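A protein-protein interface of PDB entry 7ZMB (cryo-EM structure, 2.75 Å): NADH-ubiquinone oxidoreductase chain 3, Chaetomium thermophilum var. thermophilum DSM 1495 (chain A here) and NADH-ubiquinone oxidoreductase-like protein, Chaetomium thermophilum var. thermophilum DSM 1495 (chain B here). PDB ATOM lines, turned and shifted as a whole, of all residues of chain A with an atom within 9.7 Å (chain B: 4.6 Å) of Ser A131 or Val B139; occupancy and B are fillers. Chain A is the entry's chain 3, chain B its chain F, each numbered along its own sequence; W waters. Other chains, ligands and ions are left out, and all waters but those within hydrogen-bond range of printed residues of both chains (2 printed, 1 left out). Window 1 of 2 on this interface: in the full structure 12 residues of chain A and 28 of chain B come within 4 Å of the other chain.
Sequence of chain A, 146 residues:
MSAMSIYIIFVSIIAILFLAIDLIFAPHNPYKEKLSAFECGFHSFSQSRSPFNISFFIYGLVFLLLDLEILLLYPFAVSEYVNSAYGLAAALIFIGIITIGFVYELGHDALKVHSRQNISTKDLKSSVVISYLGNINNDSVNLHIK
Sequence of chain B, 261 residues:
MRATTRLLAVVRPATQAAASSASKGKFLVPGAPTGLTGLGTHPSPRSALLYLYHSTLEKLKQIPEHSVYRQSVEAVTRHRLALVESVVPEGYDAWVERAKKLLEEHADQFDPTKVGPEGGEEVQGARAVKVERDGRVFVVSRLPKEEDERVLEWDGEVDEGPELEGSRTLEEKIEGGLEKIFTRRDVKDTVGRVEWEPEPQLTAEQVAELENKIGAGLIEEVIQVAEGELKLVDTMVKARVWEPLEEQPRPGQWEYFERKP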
ATOM      1  N   VAL A 128     -25.077  26.115 -15.956  1.00  0.00           N
ATOM      2  CA  VAL A 128     -24.843  24.709 -15.645  1.00  0.00           C
ATOM      3  C   VAL A 128     -26.191  24.085 -15.310  1.00  0.00           C
ATOM      4  O   VAL A 128     -26.776  24.357 -14.255  1.00  0.00           O
ATOM      5  CB  VAL A 128     -23.828  24.524 -14.512  1.00  0.00           C
ATOM      6  CG1 VAL A 128     -23.941  23.166 -13.906  1.00  0.00           C
ATOM      7  CG2 VAL A 128     -22.430  24.726 -15.046  1.00  0.00           C
ATOM      8  N   VAL A 129     -26.709  23.318 -16.266  1.00  0.00           N
ATOM      9  CA  VAL A 129     -27.997  22.602 -16.062  1.00  0.00           C
ATOM     10  C   VAL A 129     -27.696  21.155 -15.658  1.00  0.00           C
ATOM     11  O   VAL A 129     -26.977  20.472 -16.403  1.00  0.00           O
ATOM     12  CB  VAL A 129     -28.868  22.669 -17.332  1.00  0.00           C
ATOM     13  CG1 VAL A 129     -30.027  21.687 -17.286  1.00  0.00           C
ATOM     14  CG2 VAL A 129     -29.366  24.078 -17.605  1.00  0.00           C
ATOM     15  N   ILE A 130     -28.205  20.720 -14.507  1.00  0.00           N
ATOM     16  CA  ILE A 130     -28.045  19.310 -14.059  1.00  0.00           C
ATOM     17  C   ILE A 130     -29.279  18.542 -14.519  1.00  0.00           C
ATOM     18  O   ILE A 130     -30.345  19.142 -14.559  1.00  0.00           O
ATOM     19  CB  ILE A 130     -27.861  19.230 -12.533  1.00  0.00           C
ATOM     20  CG1 ILE A 130     -26.864  20.281 -12.036  1.00  0.00           C
ATOM     21  CG2 ILE A 130     -27.457  17.828 -12.105  1.00  0.00           C
ATOM     22  CD1 ILE A 130     -26.471  20.108 -10.594  1.00  0.00           C
ATOM     23  N   SER A 131     -29.117  17.265 -14.862  1.00  0.00           N
ATOM     24  CA  SER A 131     -30.266  16.427 -15.278  1.00  0.00           C
ATOM     25  C   SER A 131     -30.309  15.189 -14.383  1.00  0.00           C
ATOM     26  O   SER A 131     -29.237  14.766 -13.932  1.00  0.00           O
ATOM     27  CB  SER A 131     -30.200  16.090 -16.745  1.00  0.00           C
ATOM     28  OG  SER A 131     -30.516  17.218 -17.539  1.00  0.00           O
ATOM     29  N   TYR A 132     -31.494  14.643 -14.125  1.00  0.00           N
ATOM     30  CA  TYR A 132     -31.695  13.528 -13.210  1.00  0.00           C
ATOM     31  C   TYR A 132     -32.230  12.352 -14.007  1.00  0.00           C
ATOM     32  O   TYR A 132     -33.348  12.409 -14.529  1.00  0.00           O
ATOM     33  CB  TYR A 132     -32.662  13.918 -12.090  1.00  0.00           C
ATOM     34  CG  TYR A 132     -32.868  12.889 -11.004  1.00  0.00           C
ATOM     35  CD1 TYR A 132     -31.803  12.415 -10.258  1.00  0.00           C
ATOM     36  CD2 TYR A 132     -34.136  12.400 -10.719  1.00  0.00           C
ATOM     37  CE1 TYR A 132     -31.985  11.482  -9.262  1.00  0.00           C
ATOM     38  CE2 TYR A 132     -34.330  11.465  -9.723  1.00  0.00           C
ATOM     39  CZ  TYR A 132     -33.248  11.010  -8.995  1.00  0.00           C
ATOM     40  OH  TYR A 132     -33.432  10.080  -7.997  1.00  0.00           O
ATOM     41  N   LEU A 133     -31.425  11.303 -14.136  1.00  0.00           N
ATOM     42  CA  LEU A 133     -31.896  10.048 -14.695  1.00  0.00           C
ATOM     43  C   LEU A 133     -32.408   9.092 -13.634  1.00  0.00           C
ATOM     44  O   LEU A 133     -32.927   8.027 -13.978  1.00  0.00           O
ATOM     45  CB  LEU A 133     -30.791   9.365 -15.501  1.00  0.00           C
ATOM     46  CG  LEU A 133     -30.307  10.050 -16.774  1.00  0.00           C
ATOM     47  CD1 LEU A 133     -28.973   9.486 -17.216  1.00  0.00           C
ATOM     48  CD2 LEU A 133     -31.330   9.895 -17.863  1.00  0.00           C
ATOM     49  N   GLY A 134     -32.294   9.457 -12.358  1.00  0.00           N
ATOM     50  CA  GLY A 134     -32.656   8.545 -11.301  1.00  0.00           C
ATOM     51  C   GLY A 134     -31.633   7.431 -11.161  1.00  0.00           C
ATOM     52  O   GLY A 134     -30.440   7.601 -11.429  1.00  0.00           O
ATOM     53  N   ASN A 135     -32.124   6.263 -10.753  1.00  0.00           N
ATOM     54  CA  ASN A 135     -31.272   5.112 -10.512  1.00  0.00           C
ATOM     55  C   ASN A 135     -30.635   4.626 -11.814  1.00  0.00           C
ATOM     56  O   ASN A 135     -31.012   5.030 -12.917  1.00  0.00           O
ATOM     57  CB  ASN A 135     -32.074   3.985  -9.863  1.00  0.00           C
ATOM     58  CG  ASN A 135     -31.229   3.120  -8.954  1.00  0.00           C
ATOM     59  OD1 ASN A 135     -30.072   2.832  -9.253  1.00  0.00           O
ATOM     60  ND2 ASN A 135     -31.802   2.703  -7.833  1.00  0.00           N
ATOM     61  N   SER B  47     -33.512  19.026 -10.435  1.00  0.00           N
ATOM     62  CA  SER B  47     -32.318  18.145 -10.494  1.00  0.00           C
ATOM     63  C   SER B  47     -31.193  18.656  -9.591  1.00  0.00           C
ATOM     64  O   SER B  47     -30.518  17.823  -8.977  1.00  0.00           O
ATOM     65  CB  SER B  47     -31.846  17.935 -11.896  1.00  0.00           C
ATOM     66  OG  SER B  47     -32.781  17.168 -12.630  1.00  0.00           O
ATOM     67  N   TRP B  95     -38.629  11.386 -21.432  1.00  0.00           N
ATOM     68  CA  TRP B  95     -37.271  11.867 -21.654  1.00  0.00           C
ATOM     69  C   TRP B  95     -36.252  10.957 -20.988  1.00  0.00           C
ATOM     70  O   TRP B  95     -35.161  10.738 -21.527  1.00  0.00           O
ATOM     71  CB  TRP B  95     -37.125  13.302 -21.148  1.00  0.00           C
ATOM     72  CG  TRP B  95     -35.709  13.724 -21.032  1.00  0.00           C
ATOM     73  CD1 TRP B  95     -34.948  14.281 -21.998  1.00  0.00           C
ATOM     74  CD2 TRP B  95     -34.874  13.601 -19.882  1.00  0.00           C
ATOM     75  NE1 TRP B  95     -33.688  14.520 -21.531  1.00  0.00           N
ATOM     76  CE2 TRP B  95     -33.616  14.107 -20.228  1.00  0.00           C
ATOM     77  CE3 TRP B  95     -35.066  13.106 -18.592  1.00  0.00           C
ATOM     78  CZ2 TRP B  95     -32.561  14.145 -19.334  1.00  0.00           C
ATOM     79  CZ3 TRP B  95     -34.020  13.139 -17.713  1.00  0.00           C
ATOM     80  CH2 TRP B  95     -32.785  13.656 -18.082  1.00  0.00           C
ATOM     81  N   LEU B 103     -27.093   7.613 -23.063  1.00  0.00           N
ATOM     82  CA  LEU B 103     -25.945   7.361 -22.200  1.00  0.00           C
ATOM     83  C   LEU B 103     -25.396   5.958 -22.400  1.00  0.00           C
ATOM     84  O   LEU B 103     -24.177   5.757 -22.369  1.00  0.00           O
ATOM     85  CB  LEU B 103     -26.322   7.578 -20.736  1.00  0.00           C
ATOM     86  CG  LEU B 103     -26.140   8.973 -20.142  1.00  0.00           C
ATOM     87  CD1 LEU B 103     -24.680   9.354 -20.163  1.00  0.00           C
ATOM     88  CD2 LEU B 103     -26.945   9.983 -20.902  1.00  0.00           C
ATOM     89  N   ALA B 128     -21.260  17.830 -21.911  1.00  0.00           N
ATOM     90  CA  ALA B 128     -22.016  17.094 -20.903  1.00  0.00           C
ATOM     91  C   ALA B 128     -21.213  15.897 -20.412  1.00  0.00           C
ATOM     92  O   ALA B 128     -20.547  15.230 -21.201  1.00  0.00           O
ATOM     93  CB  ALA B 128     -23.365  16.619 -21.457  1.00  0.00           C
ATOM     94  N   VAL B 129     -21.288  15.632 -19.104  1.00  0.00           N
ATOM     95  CA  VAL B 129     -20.716  14.437 -18.500  1.00  0.00           C
ATOM     96  C   VAL B 129     -21.787  13.752 -17.665  1.00  0.00           C
ATOM     97  O   VAL B 129     -22.813  14.338 -17.326  1.00  0.00           O
ATOM     98  CB  VAL B 129     -19.478  14.716 -17.617  1.00  0.00           C
ATOM     99  CG1 VAL B 129     -18.436  15.444 -18.375  1.00  0.00           C
ATOM    100  CG2 VAL B 129     -19.864  15.484 -16.370  1.00  0.00           C
ATOM    101  N   LYS B 130     -21.522  12.495 -17.323  1.00  0.00           N
ATOM    102  CA  LYS B 130     -22.405  11.691 -16.490  1.00  0.00           C
ATOM    103  C   LYS B 130     -21.780  11.543 -15.110  1.00  0.00           C
ATOM    104  O   LYS B 130     -20.611  11.172 -14.994  1.00  0.00           O
ATOM    105  CB  LYS B 130     -22.650  10.319 -17.122  1.00  0.00           C
ATOM    106  CG  LYS B 130     -22.896   9.200 -16.135  1.00  0.00           C
ATOM    107  CD  LYS B 130     -23.632   8.051 -16.794  1.00  0.00           C
ATOM    108  CE  LYS B 130     -22.750   7.320 -17.792  1.00  0.00           C
ATOM    109  NZ  LYS B 130     -21.586   6.664 -17.135  1.00  0.00           N
ATOM    110  N   VAL B 137     -27.845   8.723 -11.146  1.00  0.00           N
ATOM    111  CA  VAL B 137     -27.079   9.133 -12.313  1.00  0.00           C
ATOM    112  C   VAL B 137     -27.489  10.546 -12.690  1.00  0.00           C
ATOM    113  O   VAL B 137     -28.677  10.824 -12.887  1.00  0.00           O
ATOM    114  CB  VAL B 137     -27.288   8.166 -13.492  1.00  0.00           C
ATOM    115  CG1 VAL B 137     -26.539   8.662 -14.715  1.00  0.00           C
ATOM    116  CG2 VAL B 137     -26.832   6.775 -13.111  1.00  0.00           C
ATOM    117  N   PHE B 138     -26.504  11.429 -12.811  1.00  0.00           N
ATOM    118  CA  PHE B 138     -26.727  12.812 -13.188  1.00  0.00           C
ATOM    119  C   PHE B 138     -25.929  13.130 -14.440  1.00  0.00           C
ATOM    120  O   PHE B 138     -24.847  12.582 -14.657  1.00  0.00           O
ATOM    121  CB  PHE B 138     -26.333  13.770 -12.056  1.00  0.00           C
ATOM    122  CG  PHE B 138     -27.119  13.577 -10.803  1.00  0.00           C
ATOM    123  CD1 PHE B 138     -26.702  12.686  -9.842  1.00  0.00           C
ATOM    124  CD2 PHE B 138     -28.286  14.277 -10.592  1.00  0.00           C
ATOM    125  CE1 PHE B 138     -27.431  12.502  -8.695  1.00  0.00           C
ATOM    126  CE2 PHE B 138     -29.015  14.101  -9.444  1.00  0.00           C
ATOM    127  CZ  PHE B 138     -28.586  13.213  -8.495  1.00  0.00           C
ATOM    128  N   VAL B 139     -26.476  14.008 -15.274  1.00  0.00           N
ATOM    129  CA  VAL B 139     -25.782  14.510 -16.452  1.00  0.00           C
ATOM    130  C   VAL B 139     -25.759  16.029 -16.359  1.00  0.00           C
ATOM    131  O   VAL B 139     -26.807  16.679 -16.464  1.00  0.00           O
ATOM    132  CB  VAL B 139     -26.436  14.056 -17.761  1.00  0.00           C
ATOM    133  CG1 VAL B 139     -25.785  14.752 -18.926  1.00  0.00           C
ATOM    134  CG2 VAL B 139     -26.320  12.558 -17.922  1.00  0.00           C
ATOM    135  N   VAL B 140     -24.574  16.598 -16.177  1.00  0.00           N
ATOM    136  CA  VAL B 140     -24.409  18.043 -16.094  1.00  0.00           C
ATOM    137  C   VAL B 140     -23.958  18.568 -17.451  1.00  0.00           C
ATOM    138  O   VAL B 140     -22.987  18.073 -18.034  1.00  0.00           O
ATOM    139  CB  VAL B 140     -23.432  18.432 -14.970  1.00  0.00           C
ATOM    140  CG1 VAL B 140     -22.089  17.810 -15.172  1.00  0.00           C
ATOM    141  CG2 VAL B 140     -23.275  19.922 -14.924  1.00  0.00           C
ATOM    142  N   SER B 141     -24.686  19.547 -17.969  1.00  0.00           N
ATOM    143  CA  SER B 141     -24.436  20.101 -19.288  1.00  0.00           C
ATOM    144  C   SER B 141     -24.045  21.571 -19.180  1.00  0.00           C
ATOM    145  O   SER B 141     -24.457  22.279 -18.257  1.00  0.00           O
ATOM    146  CB  SER B 141     -25.662  19.939 -20.181  1.00  0.00           C
ATOM    147  OG  SER B 141     -26.752  20.688 -19.693  1.00  0.00           O
ATOM    148  N   TRP B 196     -27.151  15.826 -26.695  1.00  0.00           N
ATOM    149  CA  TRP B 196     -27.876  15.551 -25.464  1.00  0.00           C
ATOM    150  C   TRP B 196     -28.971  16.587 -25.262  1.00  0.00           C
ATOM    151  O   TRP B 196     -28.689  17.782 -25.133  1.00  0.00           O
ATOM    152  CB  TRP B 196     -26.914  15.550 -24.280  1.00  0.00           C
ATOM    153  CG  TRP B 196     -27.571  15.805 -22.967  1.00  0.00           C
ATOM    154  CD1 TRP B 196     -27.783  17.016 -22.374  1.00  0.00           C
ATOM    155  CD2 TRP B 196     -28.099  14.824 -22.071  1.00  0.00           C
ATOM    156  NE1 TRP B 196     -28.413  16.847 -21.171  1.00  0.00           N
ATOM    157  CE2 TRP B 196     -28.615  15.508 -20.961  1.00  0.00           C
ATOM    158  CE3 TRP B 196     -28.185  13.431 -22.100  1.00  0.00           C
ATOM    159  CZ2 TRP B 196     -29.208  14.851 -19.898  1.00  0.00           C
ATOM    160  CZ3 TRP B 196     -28.775  12.783 -21.042  1.00  0.00           C
ATOM    161  CH2 TRP B 196     -29.279  13.490 -19.958  1.00  0.00           C
ATOM    162  N   PRO B 198     -31.523  18.027 -22.654  1.00  0.00           N
ATOM    163  CA  PRO B 198     -31.669  17.958 -21.196  1.00  0.00           C
ATOM    164  C   PRO B 198     -33.077  17.662 -20.704  1.00  0.00           C
ATOM    165  O   PRO B 198     -34.008  17.414 -21.474  1.00  0.00           O
ATOM    166  CB  PRO B 198     -31.208  19.349 -20.741  1.00  0.00           C
ATOM    167  CG  PRO B 198     -31.362  20.199 -21.921  1.00  0.00           C
ATOM    168  CD  PRO B 198     -31.047  19.347 -23.083  1.00  0.00           C
ATOM    169  N   GLU B 199     -33.161  17.595 -19.384  1.00  0.00           N
ATOM    170  CA  GLU B 199     -34.403  17.211 -18.685  1.00  0.00           C
ATOM    171  C   GLU B 199     -35.527  18.241 -18.794  1.00  0.00           C
ATOM    172  O   GLU B 199     -35.250  19.443 -18.713  1.00  0.00           O
ATOM    173  CB  GLU B 199     -34.046  17.042 -17.202  1.00  0.00           C
ATOM    174  CG  GLU B 199     -35.168  16.511 -16.331  1.00  0.00           C
ATOM    175  CD  GLU B 199     -34.928  16.663 -14.838  1.00  0.00           C
ATOM    176  OE1 GLU B 199     -35.160  17.769 -14.303  1.00  0.00           O
ATOM    177  OE2 GLU B 199     -34.506  15.675 -14.213  1.00  0.00           O
HETATM  178  O   HOH W   1     -32.781  19.612 -15.148  1.00  0.00           O
HETATM  179  O   HOH W   2     -29.200  12.839 -16.212  1.00  0.00           O
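N of Tyr A132 lies within hydrogen-bond range of OG of Ser B47 (3.2 Å). The backbone NH of Leu A133 sits at hydrogen-bond distance from the backbone carbonyl oxygen of Val B137 (3.1 Å). The backbone carbonyl oxygen (O) of Gly A134 lies within hydrogen-bond range of the backbone NH (N) of Val B137 (2.8 Å). The backbone NH (N) of Ser A131 lies within hydrogen-bond range of the backbone carbonyl oxygen (O) of Val B139 (2.9 Å). N of Ser B141 sits at hydrogen-bond distance from O of Val A129, at 2.9 Å. The backbone NH (N) of Glu B199 lies within hydrogen-bond range of the side-chain hydroxyl (OG) of Ser A131, 3.2 Å away. OE2 of Glu B199 is in hydrogen-bond range of N of Tyr A132 (3.2 Å).
OE2 of Glu B199 is in hydrogen-bond range of OG of Ser B47, at 2.8 Å. The indole nitrogen (NE1) of Trp B95 lies within hydrogen-bond range of the backbone carbonyl oxygen (O) of Pro B198 (2.9 Å). The backbone NH (N) of Val B140 sits at hydrogen-bond distance from the backbone carbonyl oxygen (O) of Val B129 (3.1 Å).
Val A128 touches Val B140. Val A129 touches Val B139. Val B140 touches Val A129. Phe B138 touches Ile A130. C of Ile A130 touches O of Val B139, 3.7 Å away. Ser B47 touches Ser A131 (OG to C, 3.6 Å). Ser A131 touches Trp B196. Pro B198 touches Ser A131. Trp B95 touches Tyr A132 (CZ3 to O, 3.3 Å). Phe B138 touches Tyr A132.
Ser A131 touches just these residues of chain B: Ser B47, Trp B95, Phe B138, Val B139, Trp B196, Pro B198 and Glu B199. Val B139 touches just these residues of chain A: Val A129 (3.8 Å), Ile A130 (3.7 Å) and Ser A131 (2.9 Å). Val B140 touches two residues of chain A. Printed residues of chain B within 4 Å of Leu A133: Val B137 (3.1 Å). Of the printed residues of chain B, Val A128 touches Val B140 and Ser B141. Printed residues of chain B within 4 Å of Gly A134: Val B137. Asn A135 touches none of the printed residues of chain B. Val B129 touches none of the printed residues of chain A. The nearest residue of chain B that does not touch Ser A131 is Val B137 (4.1 Å). The nearest printed residue of chain B that does not touch Leu A133 is Trp B95 (4.04 Å).
Of the 14 printed residues of chain B, 10 touch a printed residue of chain A. Hydrophobic or aromatic side chains of chain B within 4 Å of the printed part of chain A: Trp B95, Val B137, Phe B138, Val B140, Trp B196 and Pro B198. Among the printed residues, 21 pairs touch across the chains. Among the printed residues, no Asp or Glu carboxylate lies within 4 Å of a Lys or Arg side-chain nitrogen of the other chain.
Water W1 lies within hydrogen-bond range of the backbone carbonyl oxygen of Ile A130 and the side-chain carboxylate of Glu B199. Water W2 lies within hydrogen-bond range of O of Ser A131 (3.0 Å), N of Val B139 (3.1 Å) and N of Leu A133 (3.4 Å).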
